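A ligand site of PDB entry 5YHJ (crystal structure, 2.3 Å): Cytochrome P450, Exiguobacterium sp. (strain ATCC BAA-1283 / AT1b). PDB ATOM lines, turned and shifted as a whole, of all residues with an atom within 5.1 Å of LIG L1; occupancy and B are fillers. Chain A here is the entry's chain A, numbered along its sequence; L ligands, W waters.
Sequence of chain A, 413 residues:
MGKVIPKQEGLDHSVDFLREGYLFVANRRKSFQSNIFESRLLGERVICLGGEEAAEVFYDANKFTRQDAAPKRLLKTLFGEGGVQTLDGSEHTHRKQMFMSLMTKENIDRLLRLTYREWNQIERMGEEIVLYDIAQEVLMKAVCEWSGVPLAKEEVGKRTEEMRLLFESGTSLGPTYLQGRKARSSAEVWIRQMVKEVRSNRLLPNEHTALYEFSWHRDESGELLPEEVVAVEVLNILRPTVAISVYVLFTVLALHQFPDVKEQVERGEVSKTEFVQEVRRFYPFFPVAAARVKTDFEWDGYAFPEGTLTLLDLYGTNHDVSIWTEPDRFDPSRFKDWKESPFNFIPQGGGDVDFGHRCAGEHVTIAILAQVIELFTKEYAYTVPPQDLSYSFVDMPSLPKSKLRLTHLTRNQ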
ATOM      1  N   PHE A  58      -4.833   0.570  17.089  1.00  0.00           N
ATOM      2  CA  PHE A  58      -3.739   1.437  16.661  1.00  0.00           C
ATOM      3  C   PHE A  58      -4.214   2.838  16.287  1.00  0.00           C
ATOM      4  O   PHE A  58      -3.453   3.808  16.437  1.00  0.00           O
ATOM      5  CB  PHE A  58      -3.037   0.753  15.492  1.00  0.00           C
ATOM      6  CG  PHE A  58      -1.866   1.509  14.925  1.00  0.00           C
ATOM      7  CD1 PHE A  58      -0.584   1.262  15.390  1.00  0.00           C
ATOM      8  CD2 PHE A  58      -2.037   2.390  13.884  1.00  0.00           C
ATOM      9  CE1 PHE A  58       0.493   1.932  14.835  1.00  0.00           C
ATOM     10  CE2 PHE A  58      -0.981   3.048  13.358  1.00  0.00           C
ATOM     11  CZ  PHE A  58       0.278   2.830  13.817  1.00  0.00           C
ATOM     12  N   TYR A  59      -5.448   2.980  15.767  1.00  0.00           N
ATOM     13  CA  TYR A  59      -6.004   4.276  15.404  1.00  0.00           C
ATOM     14  C   TYR A  59      -6.893   4.854  16.504  1.00  0.00           C
ATOM     15  O   TYR A  59      -7.654   5.791  16.251  1.00  0.00           O
ATOM     16  CB  TYR A  59      -6.769   4.222  14.071  1.00  0.00           C
ATOM     17  CG  TYR A  59      -5.839   4.117  12.862  1.00  0.00           C
ATOM     18  CD1 TYR A  59      -5.135   5.223  12.403  1.00  0.00           C
ATOM     19  CD2 TYR A  59      -5.640   2.903  12.213  1.00  0.00           C
ATOM     20  CE1 TYR A  59      -4.252   5.122  11.335  1.00  0.00           C
ATOM     21  CE2 TYR A  59      -4.762   2.794  11.141  1.00  0.00           C
ATOM     22  CZ  TYR A  59      -4.070   3.912  10.700  1.00  0.00           C
ATOM     23  OH  TYR A  59      -3.214   3.808   9.621  1.00  0.00           O
ATOM     24  N   ARG A  66       1.283   9.782  17.401  1.00  0.00           N
ATOM     25  CA  ARG A  66       2.300   9.850  16.358  1.00  0.00           C
ATOM     26  C   ARG A  66       3.431  10.796  16.734  1.00  0.00           C
ATOM     27  O   ARG A  66       4.397  10.915  15.965  1.00  0.00           O
ATOM     28  CB  ARG A  66       1.661  10.260  15.016  1.00  0.00           C
ATOM     29  CG  ARG A  66       0.444   9.418  14.609  1.00  0.00           C
ATOM     30  CD  ARG A  66       0.720   7.897  14.674  1.00  0.00           C
ATOM     31  NE  ARG A  66      -0.370   7.141  14.064  1.00  0.00           N
ATOM     32  CZ  ARG A  66      -0.480   6.930  12.745  1.00  0.00           C
ATOM     33  NH1 ARG A  66      -1.514   6.264  12.252  1.00  0.00           N
ATOM     34  NH2 ARG A  66       0.450   7.394  11.924  1.00  0.00           N
ATOM     35  N   VAL A  84       2.209  17.287   8.558  1.00  0.00           N
ATOM     36  CA  VAL A  84       0.994  16.843   9.246  1.00  0.00           C
ATOM     37  C   VAL A  84       1.199  15.459   9.873  1.00  0.00           C
ATOM     38  O   VAL A  84       0.553  15.125  10.890  1.00  0.00           O
ATOM     39  CB  VAL A  84      -0.196  16.866   8.274  1.00  0.00           C
ATOM     40  CG1 VAL A  84      -0.069  15.775   7.212  1.00  0.00           C
ATOM     41  CG2 VAL A  84      -1.523  16.774   9.030  1.00  0.00           C
ATOM     42  N   GLN A  85       2.126  14.669   9.325  1.00  0.00           N
ATOM     43  CA  GLN A  85       2.396  13.331   9.869  1.00  0.00           C
ATOM     44  C   GLN A  85       2.769  13.415  11.338  1.00  0.00           C
ATOM     45  O   GLN A  85       2.425  12.532  12.131  1.00  0.00           O
ATOM     46  CB  GLN A  85       3.534  12.642   9.107  1.00  0.00           C
ATOM     47  CG  GLN A  85       3.230  12.253   7.696  1.00  0.00           C
ATOM     48  CD  GLN A  85       3.652  13.317   6.694  1.00  0.00           C
ATOM     49  OE1 GLN A  85       4.065  14.428   7.065  1.00  0.00           O
ATOM     50  NE2 GLN A  85       3.576  12.982   5.413  1.00  0.00           N
ATOM     51  N   HIS A  92      -3.288  18.944  14.806  1.00  0.00           N
ATOM     52  CA  HIS A  92      -3.334  18.003  13.697  1.00  0.00           C
ATOM     53  C   HIS A  92      -4.666  18.037  12.988  1.00  0.00           C
ATOM     54  O   HIS A  92      -4.730  17.880  11.769  1.00  0.00           O
ATOM     55  CB  HIS A  92      -3.059  16.585  14.190  1.00  0.00           C
ATOM     56  CG  HIS A  92      -3.304  15.560  13.124  1.00  0.00           C
ATOM     57  ND1 HIS A  92      -4.540  15.003  12.923  1.00  0.00           N
ATOM     58  CD2 HIS A  92      -2.500  15.074  12.165  1.00  0.00           C
ATOM     59  CE1 HIS A  92      -4.483  14.177  11.894  1.00  0.00           C
ATOM     60  NE2 HIS A  92      -3.254  14.198  11.413  1.00  0.00           N
ATOM     61  N   LYS A  96      -4.958  18.914   9.102  1.00  0.00           N
ATOM     62  CA  LYS A  96      -5.578  17.896   8.260  1.00  0.00           C
ATOM     63  C   LYS A  96      -6.796  18.436   7.519  1.00  0.00           C
ATOM     64  O   LYS A  96      -7.070  18.018   6.392  1.00  0.00           O
ATOM     65  CB  LYS A  96      -5.971  16.681   9.108  1.00  0.00           C
ATOM     66  CG  LYS A  96      -6.438  15.485   8.289  1.00  0.00           C
ATOM     67  CD  LYS A  96      -5.342  15.007   7.331  1.00  0.00           C
ATOM     68  CE  LYS A  96      -5.620  13.618   6.749  1.00  0.00           C
ATOM     69  NZ  LYS A  96      -5.598  12.578   7.848  1.00  0.00           N
ATOM     70  N   PHE A  99      -5.416  19.997   4.484  1.00  0.00           N
ATOM     71  CA  PHE A  99      -5.226  19.120   3.330  1.00  0.00           C
ATOM     72  C   PHE A  99      -6.561  18.731   2.706  1.00  0.00           C
ATOM     73  O   PHE A  99      -6.700  18.763   1.475  1.00  0.00           O
ATOM     74  CB  PHE A  99      -4.429  17.877   3.721  1.00  0.00           C
ATOM     75  CG  PHE A  99      -2.950  18.085   3.722  1.00  0.00           C
ATOM     76  CD1 PHE A  99      -2.330  18.696   4.813  1.00  0.00           C
ATOM     77  CD2 PHE A  99      -2.163  17.651   2.667  1.00  0.00           C
ATOM     78  CE1 PHE A  99      -0.962  18.877   4.832  1.00  0.00           C
ATOM     79  CE2 PHE A  99      -0.810  17.841   2.658  1.00  0.00           C
ATOM     80  CZ  PHE A  99      -0.200  18.460   3.743  1.00  0.00           C
ATOM     81  N   MET A 103      -9.352  18.306  -1.458  1.00  0.00           N
ATOM     82  CA  MET A 103      -9.907  17.078  -1.995  1.00  0.00           C
ATOM     83  C   MET A 103     -11.400  17.171  -2.239  1.00  0.00           C
ATOM     84  O   MET A 103     -12.148  16.201  -2.090  1.00  0.00           O
ATOM     85  CB  MET A 103      -9.563  15.920  -1.047  1.00  0.00           C
ATOM     86  CG  MET A 103      -8.083  15.941  -0.613  1.00  0.00           C
ATOM     87  SD  MET A 103      -6.883  15.946  -1.969  1.00  0.00           S
ATOM     88  CE  MET A 103      -5.320  16.215  -1.132  1.00  0.00           C
ATOM     89  N   ASN A 236       4.464  17.142   0.536  1.00  0.00           N
ATOM     90  CA  ASN A 236       3.543  16.071   0.873  1.00  0.00           C
ATOM     91  C   ASN A 236       2.303  16.043   0.004  1.00  0.00           C
ATOM     92  O   ASN A 236       1.336  15.344   0.325  1.00  0.00           O
ATOM     93  CB  ASN A 236       3.144  16.174   2.349  1.00  0.00           C
ATOM     94  CG  ASN A 236       4.297  15.928   3.282  1.00  0.00           C
ATOM     95  OD1 ASN A 236       5.336  15.410   2.867  1.00  0.00           O
ATOM     96  ND2 ASN A 236       4.134  16.327   4.547  1.00  0.00           N
ATOM     97  N   ILE A 237       2.269  16.813  -1.091  1.00  0.00           N
ATOM     98  CA  ILE A 237       1.332  16.566  -2.169  1.00  0.00           C
ATOM     99  C   ILE A 237       2.058  16.237  -3.469  1.00  0.00           C
ATOM    100  O   ILE A 237       1.667  15.294  -4.172  1.00  0.00           O
ATOM    101  CB  ILE A 237       0.371  17.753  -2.373  1.00  0.00           C
ATOM    102  CG1 ILE A 237      -0.749  17.609  -1.358  1.00  0.00           C
ATOM    103  CG2 ILE A 237      -0.166  17.806  -3.841  1.00  0.00           C
ATOM    104  CD1 ILE A 237      -1.384  18.882  -0.980  1.00  0.00           C
ATOM    105  N   PRO A 240       3.830  12.218  -3.177  1.00  0.00           N
ATOM    106  CA  PRO A 240       3.049  10.974  -3.270  1.00  0.00           C
ATOM    107  C   PRO A 240       2.213  10.902  -4.550  1.00  0.00           C
ATOM    108  O   PRO A 240       1.938   9.792  -5.031  1.00  0.00           O
ATOM    109  CB  PRO A 240       2.187  10.982  -1.991  1.00  0.00           C
ATOM    110  CG  PRO A 240       2.448  12.331  -1.293  1.00  0.00           C
ATOM    111  CD  PRO A 240       3.198  13.198  -2.272  1.00  0.00           C
ATOM    112  N   THR A 241       1.816  12.043  -5.123  1.00  0.00           N
ATOM    113  CA  THR A 241       1.140  12.031  -6.421  1.00  0.00           C
ATOM    114  C   THR A 241       2.008  11.392  -7.493  1.00  0.00           C
ATOM    115  O   THR A 241       1.545  10.558  -8.260  1.00  0.00           O
ATOM    116  CB  THR A 241       0.737  13.450  -6.849  1.00  0.00           C
ATOM    117  OG1 THR A 241       0.057  14.099  -5.776  1.00  0.00           O
ATOM    118  CG2 THR A 241      -0.211  13.395  -8.067  1.00  0.00           C
ATOM    119  N   ALA A 243       4.400   9.316  -6.735  1.00  0.00           N
ATOM    120  CA  ALA A 243       4.463   7.927  -6.299  1.00  0.00           C
ATOM    121  C   ALA A 243       3.307   7.075  -6.828  1.00  0.00           C
ATOM    122  O   ALA A 243       3.453   5.863  -6.947  1.00  0.00           O
ATOM    123  CB  ALA A 243       4.512   7.842  -4.762  1.00  0.00           C
ATOM    124  N   ILE A 244       2.165   7.689  -7.183  1.00  0.00           N
ATOM    125  CA  ILE A 244       1.047   6.954  -7.803  1.00  0.00           C
ATOM    126  C   ILE A 244       1.517   6.165  -9.037  1.00  0.00           C
ATOM    127  O   ILE A 244       0.904   5.158  -9.396  1.00  0.00           O
ATOM    128  CB  ILE A 244      -0.130   7.890  -8.132  1.00  0.00           C
ATOM    129  CG1 ILE A 244      -0.670   8.498  -6.846  1.00  0.00           C
ATOM    130  CG2 ILE A 244      -1.277   7.175  -8.874  1.00  0.00           C
ATOM    131  CD1 ILE A 244      -1.720   9.614  -7.077  1.00  0.00           C
ATOM    132  N   TYR A 247       1.466   2.421  -8.483  1.00  0.00           N
ATOM    133  CA  TYR A 247       0.137   1.857  -8.713  1.00  0.00           C
ATOM    134  C   TYR A 247      -0.266   1.879 -10.184  1.00  0.00           C
ATOM    135  O   TYR A 247      -1.014   0.999 -10.616  1.00  0.00           O
ATOM    136  CB  TYR A 247      -0.882   2.608  -7.887  1.00  0.00           C
ATOM    137  CG  TYR A 247      -1.063   2.113  -6.463  1.00  0.00           C
ATOM    138  CD1 TYR A 247      -0.890   0.769  -6.114  1.00  0.00           C
ATOM    139  CD2 TYR A 247      -1.460   3.002  -5.476  1.00  0.00           C
ATOM    140  CE1 TYR A 247      -1.078   0.347  -4.787  1.00  0.00           C
ATOM    141  CE2 TYR A 247      -1.650   2.592  -4.177  1.00  0.00           C
ATOM    142  CZ  TYR A 247      -1.469   1.273  -3.839  1.00  0.00           C
ATOM    143  OH  TYR A 247      -1.695   0.958  -2.535  1.00  0.00           O
ATOM    144  N   PHE A 285       2.650  -2.040  -1.449  1.00  0.00           N
ATOM    145  CA  PHE A 285       3.233  -0.720  -1.627  1.00  0.00           C
ATOM    146  C   PHE A 285       3.704  -0.127  -0.287  1.00  0.00           C
ATOM    147  O   PHE A 285       4.905  -0.135   0.000  1.00  0.00           O
ATOM    148  CB  PHE A 285       2.215   0.220  -2.302  1.00  0.00           C
ATOM    149  CG  PHE A 285       2.819   1.494  -2.894  1.00  0.00           C
ATOM    150  CD1 PHE A 285       4.112   1.885  -2.589  1.00  0.00           C
ATOM    151  CD2 PHE A 285       2.072   2.268  -3.772  1.00  0.00           C
ATOM    152  CE1 PHE A 285       4.646   3.061  -3.144  1.00  0.00           C
ATOM    153  CE2 PHE A 285       2.571   3.437  -4.317  1.00  0.00           C
ATOM    154  CZ  PHE A 285       3.868   3.840  -4.018  1.00  0.00           C
ATOM    155  N   PHE A 286       2.800   0.436   0.495  1.00  0.00           N
ATOM    156  CA  PHE A 286       3.165   0.912   1.821  1.00  0.00           C
ATOM    157  C   PHE A 286       3.134  -0.254   2.796  1.00  0.00           C
ATOM    158  O   PHE A 286       2.061  -0.861   2.969  1.00  0.00           O
ATOM    159  CB  PHE A 286       2.210   2.028   2.261  1.00  0.00           C
ATOM    160  CG  PHE A 286       2.839   3.018   3.212  1.00  0.00           C
ATOM    161  CD1 PHE A 286       3.269   2.634   4.473  1.00  0.00           C
ATOM    162  CD2 PHE A 286       3.027   4.341   2.835  1.00  0.00           C
ATOM    163  CE1 PHE A 286       3.870   3.537   5.317  1.00  0.00           C
ATOM    164  CE2 PHE A 286       3.606   5.245   3.681  1.00  0.00           C
ATOM    165  CZ  PHE A 286       4.035   4.841   4.932  1.00  0.00           C
ATOM    166  N   ALA A 289       2.332   1.178   8.948  1.00  0.00           N
ATOM    167  CA  ALA A 289       2.191   2.463   9.637  1.00  0.00           C
ATOM    168  C   ALA A 289       2.821   2.383  11.039  1.00  0.00           C
ATOM    169  O   ALA A 289       2.955   1.311  11.623  1.00  0.00           O
ATOM    170  CB  ALA A 289       0.726   2.876   9.769  1.00  0.00           C
ATOM    171  N   LEU A 314       0.009  -3.020   7.118  1.00  0.00           N
ATOM    172  CA  LEU A 314      -1.020  -2.660   6.152  1.00  0.00           C
ATOM    173  C   LEU A 314      -1.201  -3.751   5.093  1.00  0.00           C
ATOM    174  O   LEU A 314      -2.317  -4.236   4.872  1.00  0.00           O
ATOM    175  CB  LEU A 314      -0.664  -1.327   5.487  1.00  0.00           C
ATOM    176  CG  LEU A 314      -0.261  -0.153   6.390  1.00  0.00           C
ATOM    177  CD1 LEU A 314       0.116   1.014   5.531  1.00  0.00           C
ATOM    178  CD2 LEU A 314      -1.381   0.256   7.338  1.00  0.00           C
ATOM    179  N   PRO A 347      -4.820   0.001   2.685  1.00  0.00           N
ATOM    180  CA  PRO A 347      -3.592   0.234   1.917  1.00  0.00           C
ATOM    181  C   PRO A 347      -3.043   1.640   2.051  1.00  0.00           C
ATOM    182  O   PRO A 347      -1.835   1.853   1.876  1.00  0.00           O
ATOM    183  CB  PRO A 347      -4.023  -0.063   0.472  1.00  0.00           C
ATOM    184  CG  PRO A 347      -5.502   0.322   0.457  1.00  0.00           C
ATOM    185  CD  PRO A 347      -5.997  -0.143   1.822  1.00  0.00           C
ATOM    186  N   GLN A 348      -3.863   2.609   2.410  1.00  0.00           N
ATOM    187  CA  GLN A 348      -3.369   3.956   2.642  1.00  0.00           C
ATOM    188  C   GLN A 348      -3.757   4.421   4.047  1.00  0.00           C
ATOM    189  O   GLN A 348      -4.163   5.567   4.279  1.00  0.00           O
ATOM    190  CB  GLN A 348      -3.866   4.885   1.518  1.00  0.00           C
ATOM    191  CG  GLN A 348      -3.298   4.430   0.125  1.00  0.00           C
ATOM    192  CD  GLN A 348      -3.770   5.263  -1.104  1.00  0.00           C
ATOM    193  OE1 GLN A 348      -4.361   4.730  -2.037  1.00  0.00           O
ATOM    194  NE2 GLN A 348      -3.463   6.558  -1.093  1.00  0.00           N
ATOM    195  N   GLY A 349      -3.608   3.529   5.029  1.00  0.00           N
ATOM    196  CA  GLY A 349      -3.956   3.864   6.389  1.00  0.00           C
ATOM    197  C   GLY A 349      -5.388   3.497   6.743  1.00  0.00           C
ATOM    198  O   GLY A 349      -6.242   3.276   5.893  1.00  0.00           O
ATOM    199  N   GLY A 350      -5.655   3.428   8.057  1.00  0.00           N
ATOM    200  CA  GLY A 350      -6.973   3.170   8.576  1.00  0.00           C
ATOM    201  C   GLY A 350      -7.523   4.352   9.361  1.00  0.00           C
ATOM    202  O   GLY A 350      -6.878   5.388   9.519  1.00  0.00           O
ATOM    203  N   GLY A 356      -8.109  11.401  12.165  1.00  0.00           N
ATOM    204  CA  GLY A 356      -6.937  10.567  12.322  1.00  0.00           C
ATOM    205  C   GLY A 356      -5.957  10.761  11.187  1.00  0.00           C
ATOM    206  O   GLY A 356      -6.185  11.558  10.277  1.00  0.00           O
ATOM    207  N   HIS A 357      -4.851   9.997  11.249  1.00  0.00           N
ATOM    208  CA  HIS A 357      -3.697  10.153  10.360  1.00  0.00           C
ATOM    209  C   HIS A 357      -3.826   9.391   9.044  1.00  0.00           C
ATOM    210  O   HIS A 357      -2.823   9.243   8.321  1.00  0.00           O
ATOM    211  CB  HIS A 357      -2.411   9.716  11.056  1.00  0.00           C
ATOM    212  CG  HIS A 357      -1.716  10.796  11.822  1.00  0.00           C
ATOM    213  ND1 HIS A 357      -2.238  11.367  12.967  1.00  0.00           N
ATOM    214  CD2 HIS A 357      -0.510  11.381  11.627  1.00  0.00           C
ATOM    215  CE1 HIS A 357      -1.391  12.257  13.439  1.00  0.00           C
ATOM    216  NE2 HIS A 357      -0.334  12.294  12.645  1.00  0.00           N
ATOM    217  N   ARG A 358      -5.013   8.885   8.741  1.00  0.00           N
ATOM    218  CA  ARG A 358      -5.257   8.205   7.485  1.00  0.00           C
ATOM    219  C   ARG A 358      -4.811   9.089   6.316  1.00  0.00           C
ATOM    220  O   ARG A 358      -4.770  10.319   6.418  1.00  0.00           O
ATOM    221  CB  ARG A 358      -6.738   7.844   7.377  1.00  0.00           C
ATOM    222  CG  ARG A 358      -7.149   7.100   6.126  1.00  0.00           C
ATOM    223  CD  ARG A 358      -8.608   6.711   6.169  1.00  0.00           C
ATOM    224  NE  ARG A 358      -8.926   5.727   5.140  1.00  0.00           N
ATOM    225  CZ  ARG A 358      -9.612   4.607   5.345  1.00  0.00           C
ATOM    226  NH1 ARG A 358     -10.096   4.314   6.558  1.00  0.00           N
ATOM    227  NH2 ARG A 358      -9.832   3.797   4.325  1.00  0.00           N
ATOM    228  N   CYS A 359      -4.431   8.437   5.211  1.00  0.00           N
ATOM    229  CA  CYS A 359      -3.902   9.132   4.045  1.00  0.00           C
ATOM    230  C   CYS A 359      -4.861  10.197   3.515  1.00  0.00           C
ATOM    231  O   CYS A 359      -6.072   9.972   3.405  1.00  0.00           O
ATOM    232  CB  CYS A 359      -3.602   8.146   2.930  1.00  0.00           C
ATOM    233  SG  CYS A 359      -3.383   8.854   1.305  1.00  0.00           S
ATOM    234  N   ALA A 360      -4.295  11.351   3.169  1.00  0.00           N
ATOM    235  CA  ALA A 360      -5.067  12.459   2.622  1.00  0.00           C
ATOM    236  C   ALA A 360      -5.485  12.249   1.161  1.00  0.00           C
ATOM    237  O   ALA A 360      -6.471  12.847   0.708  1.00  0.00           O
ATOM    238  CB  ALA A 360      -4.240  13.744   2.729  1.00  0.00           C
ATOM    239  N   GLY A 361      -4.766  11.398   0.412  1.00  0.00           N
ATOM    240  CA  GLY A 361      -4.841  11.428  -1.050  1.00  0.00           C
ATOM    241  C   GLY A 361      -5.526  10.238  -1.692  1.00  0.00           C
ATOM    242  O   GLY A 361      -5.198   9.877  -2.818  1.00  0.00           O
ATOM    243  N   VAL A 364      -7.807  11.067  -4.656  1.00  0.00           N
ATOM    244  CA  VAL A 364      -6.923  11.388  -5.776  1.00  0.00           C
ATOM    245  C   VAL A 364      -6.331  10.127  -6.381  1.00  0.00           C
ATOM    246  O   VAL A 364      -6.351   9.920  -7.604  1.00  0.00           O
ATOM    247  CB  VAL A 364      -5.831  12.378  -5.332  1.00  0.00           C
ATOM    248  CG1 VAL A 364      -4.737  12.408  -6.366  1.00  0.00           C
ATOM    249  CG2 VAL A 364      -6.429  13.766  -5.156  1.00  0.00           C
ATOM    250  N   THR A 365      -5.793   9.238  -5.519  1.00  0.00           N
ATOM    251  CA  THR A 365      -5.182   7.984  -5.964  1.00  0.00           C
ATOM    252  C   THR A 365      -6.167   7.159  -6.795  1.00  0.00           C
ATOM    253  O   THR A 365      -5.851   6.679  -7.889  1.00  0.00           O
ATOM    254  CB  THR A 365      -4.702   7.175  -4.747  1.00  0.00           C
ATOM    255  OG1 THR A 365      -3.916   7.990  -3.872  1.00  0.00           O
ATOM    256  CG2 THR A 365      -3.840   5.996  -5.200  1.00  0.00           C
HETATM  257  C1  LIG L   1      -0.325   9.361   4.763  1.00  0.00           C
HETATM  258  C2  LIG L   1      -1.155  12.436   1.117  1.00  0.00           C
HETATM  259  C3  LIG L   1      -0.744   8.807  -2.067  1.00  0.00           C
HETATM  260  C4  LIG L   1      -0.405   5.645   1.577  1.00  0.00           C
HETATM  261  C5  LIG L   1      -0.544  10.523   4.062  1.00  0.00           C
HETATM  262  C6  LIG L   1      -0.619  11.865   4.618  1.00  0.00           C
HETATM  263  C7  LIG L   1      -0.852  12.722   3.603  1.00  0.00           C
HETATM  264  C8  LIG L   1      -0.923  11.948   2.377  1.00  0.00           C
HETATM  265  C9  LIG L   1      -1.000  14.252   3.710  1.00  0.00           C
HETATM  266  C10 LIG L   1      -0.479  12.246   6.105  1.00  0.00           C
HETATM  267  C11 LIG L   1      -1.869  12.108   6.766  1.00  0.00           C
HETATM  268  C12 LIG L   1      -1.893  12.558   8.211  1.00  0.00           C
HETATM  269  O1  LIG L   1      -0.802  12.693   8.811  1.00  0.00           O
HETATM  270  O2  LIG L   1      -2.998  12.781   8.790  1.00  0.00           O
HETATM  271  C13 LIG L   1      -1.150  11.721  -0.065  1.00  0.00           C
HETATM  272  C14 LIG L   1      -1.440  12.249  -1.390  1.00  0.00           C
HETATM  273  C15 LIG L   1      -1.313  11.226  -2.264  1.00  0.00           C
HETATM  274  C16 LIG L   1      -0.965  10.044  -1.527  1.00  0.00           C
HETATM  275  C17 LIG L   1      -1.798  13.731  -1.657  1.00  0.00           C
HETATM  276  C18 LIG L   1      -1.503  11.181  -3.796  1.00  0.00           C
HETATM  277  C19 LIG L   1      -1.968  12.204  -4.521  1.00  0.00           C
HETATM  278  C20 LIG L   1      -0.522   7.641  -1.391  1.00  0.00           C
HETATM  279  C21 LIG L   1      -0.089   6.393  -1.975  1.00  0.00           C
HETATM  280  C22 LIG L   1       0.006   5.507  -0.986  1.00  0.00           C
HETATM  281  C23 LIG L   1      -0.352   6.150   0.280  1.00  0.00           C
HETATM  282  C24 LIG L   1       0.193   6.162  -3.481  1.00  0.00           C
HETATM  283  C25 LIG L   1       0.449   4.053  -1.225  1.00  0.00           C
HETATM  284  C26 LIG L   1       0.291   3.110  -0.298  1.00  0.00           C
HETATM  285  C27 LIG L   1      -0.341   6.379   2.763  1.00  0.00           C
HETATM  286  C28 LIG L   1      -0.210   5.836   4.116  1.00  0.00           C
HETATM  287  C29 LIG L   1      -0.184   6.865   4.991  1.00  0.00           C
HETATM  288  C30 LIG L   1      -0.301   8.093   4.225  1.00  0.00           C
HETATM  289  C31 LIG L   1      -0.107   4.351   4.458  1.00  0.00           C
HETATM  290  C32 LIG L   1      -0.004   6.812   6.532  1.00  0.00           C
HETATM  291  C33 LIG L   1      -1.234   6.374   7.313  1.00  0.00           C
HETATM  292  C34 LIG L   1      -1.020   6.574   8.796  1.00  0.00           C
HETATM  293  O3  LIG L   1      -1.881   6.135   9.579  1.00  0.00           O
HETATM  294  O4  LIG L   1       0.009   7.174   9.191  1.00  0.00           O
HETATM  295  N1  LIG L   1      -0.739  10.621   2.700  1.00  0.00           N
HETATM  296  N2  LIG L   1      -0.863  10.382  -0.203  1.00  0.00           N
HETATM  297  N3  LIG L   1      -0.670   7.454  -0.032  1.00  0.00           N
HETATM  298  N4  LIG L   1      -0.395   7.752   2.897  1.00  0.00           N
HETATM  299 FE1  LIG L   1      -0.939   9.032   1.345  1.00  0.00          FE
HETATM  300  C1  LG2 L   2       4.569   9.016   0.113  1.00  0.00           C
HETATM  301  O1  LG2 L   2       4.307   9.502   1.261  1.00  0.00           O
HETATM  302  O2  LG2 L   2       5.364   9.651  -0.626  1.00  0.00           O
HETATM  303  C2  LG2 L   2       3.802   7.813  -0.439  1.00  0.00           C
HETATM  304  C3  LG2 L   2       4.753   6.898  -1.195  1.00  0.00           C
HETATM  305  C4  LG2 L   2       4.780   5.519  -0.561  1.00  0.00           C
HETATM  306  C5  LG2 L   2       6.164   4.900  -0.418  1.00  0.00           C
HETATM  307  C6  LG2 L   2       6.187   3.900   0.733  1.00  0.00           C
HETATM  308  C7  LG2 L   2       7.203   2.776   0.540  1.00  0.00           C
HETATM  309  C8  LG2 L   2       8.556   3.099   1.175  1.00  0.00           C
HETATM  310  C9  LG2 L   2       9.068   1.922   1.988  1.00  0.00           C
HETATM  311  C10 LG2 L   2       9.428   2.285   3.438  1.00  0.00           C
HETATM  312  C11 LG2 L   2       8.240   2.780   4.255  1.00  0.00           C
HETATM  313  C12 LG2 L   2       8.431   2.491   5.748  1.00  0.00           C
HETATM  314  C13 LG2 L   2       7.449   3.227   6.642  1.00  0.00           C
HETATM  315  C14 LG2 L   2       7.833   3.070   8.106  1.00  0.00           C
HETATM  316  O   HOH W   1       0.943   9.125   1.045  1.00  0.00           O
HETATM  317  O   HOH W   2       0.196   9.763   8.691  1.00  0.00           O
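O of Val 84 sits close to O1 of LIG L1, 3.5 Å away. N3 of LIG L1 sits close to NE2 of Gln 348. O of His 357 lies close to O3 of LIG L1. Merely in contact with LIG L1: Gln 85, Phe 99, Asn 236, Pro 240, Thr 241, Ile 244, Tyr 247, Phe 285, Phe 286, Leu 314, Pro 347, Gly 349, Gly 356, Arg 358, Ala 360, Gly 361, Val 364 and Thr 365. Hydrophobic or aromatic side chains that line LIG L1: Tyr 59, Val 84, His 92, Phe 99, Pro 240, Ile 244, Tyr 247, Phe 285, Phe 286, Leu 314, His 357, Ala 360 and Val 364. The nearest printed residue that does not touch LIG L1 is Ile 237 (4.03 Å).
A ring nitrogen (ND1) of His 357 lies close to a ring nitrogen (NE2) of His 92 (3.4 Å). The side-chain hydroxyl (OG1) of Thr 241 is in hydrogen-bond range of the backbone carbonyl oxygen (O) of Ile 237, 2.6 Å away. NZ of Lys 96 sits at hydrogen-bond distance from O of Gly 356 (2.7 Å). The side-chain amide oxygen (OE1) of Gln 85 is in hydrogen-bond range of the side-chain amide nitrogen (ND2) of Asn 236, at 3.2 Å. The side-chain hydroxyl (OG1) of Thr 365 sits at hydrogen-bond distance from the side-chain amide nitrogen (NE2) of Gln 348 (3.2 Å). A ring nitrogen (NE2) of His 357 is in hydrogen-bond range of the backbone carbonyl oxygen (O) of Gln 85. The backbone carbonyl oxygen (O) of Gly 361 lies within hydrogen-bond range of the side-chain hydroxyl (OG1) of Thr 365 (2.5 Å). N of Gly 350 is in hydrogen-bond range of OH of Tyr 59, 2.9 Å away.
The side-chain hydroxyl (OH) of Tyr 59 sits at hydrogen-bond distance from an oxygen (O3) of LIG L1 (2.7 Å). NH1 of Arg 66 lies within salt-bridge range of O3 of LIG L1. SG of Cys 359 binds FE1 of LIG L1. An oxygen (O2) of LIG L1 is in salt-bridge range of the side-chain amino group (NZ) of Lys 96, at 2.8 Å. An oxygen (O2) of LIG L1 lies within hydrogen-bond range of a ring nitrogen (NE2) of His 92, 3.0 Å away.
Water W2 lies within hydrogen-bond range of an oxygen (O4) of LIG L1 and the backbone carbonyl oxygen (O) of His 357.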
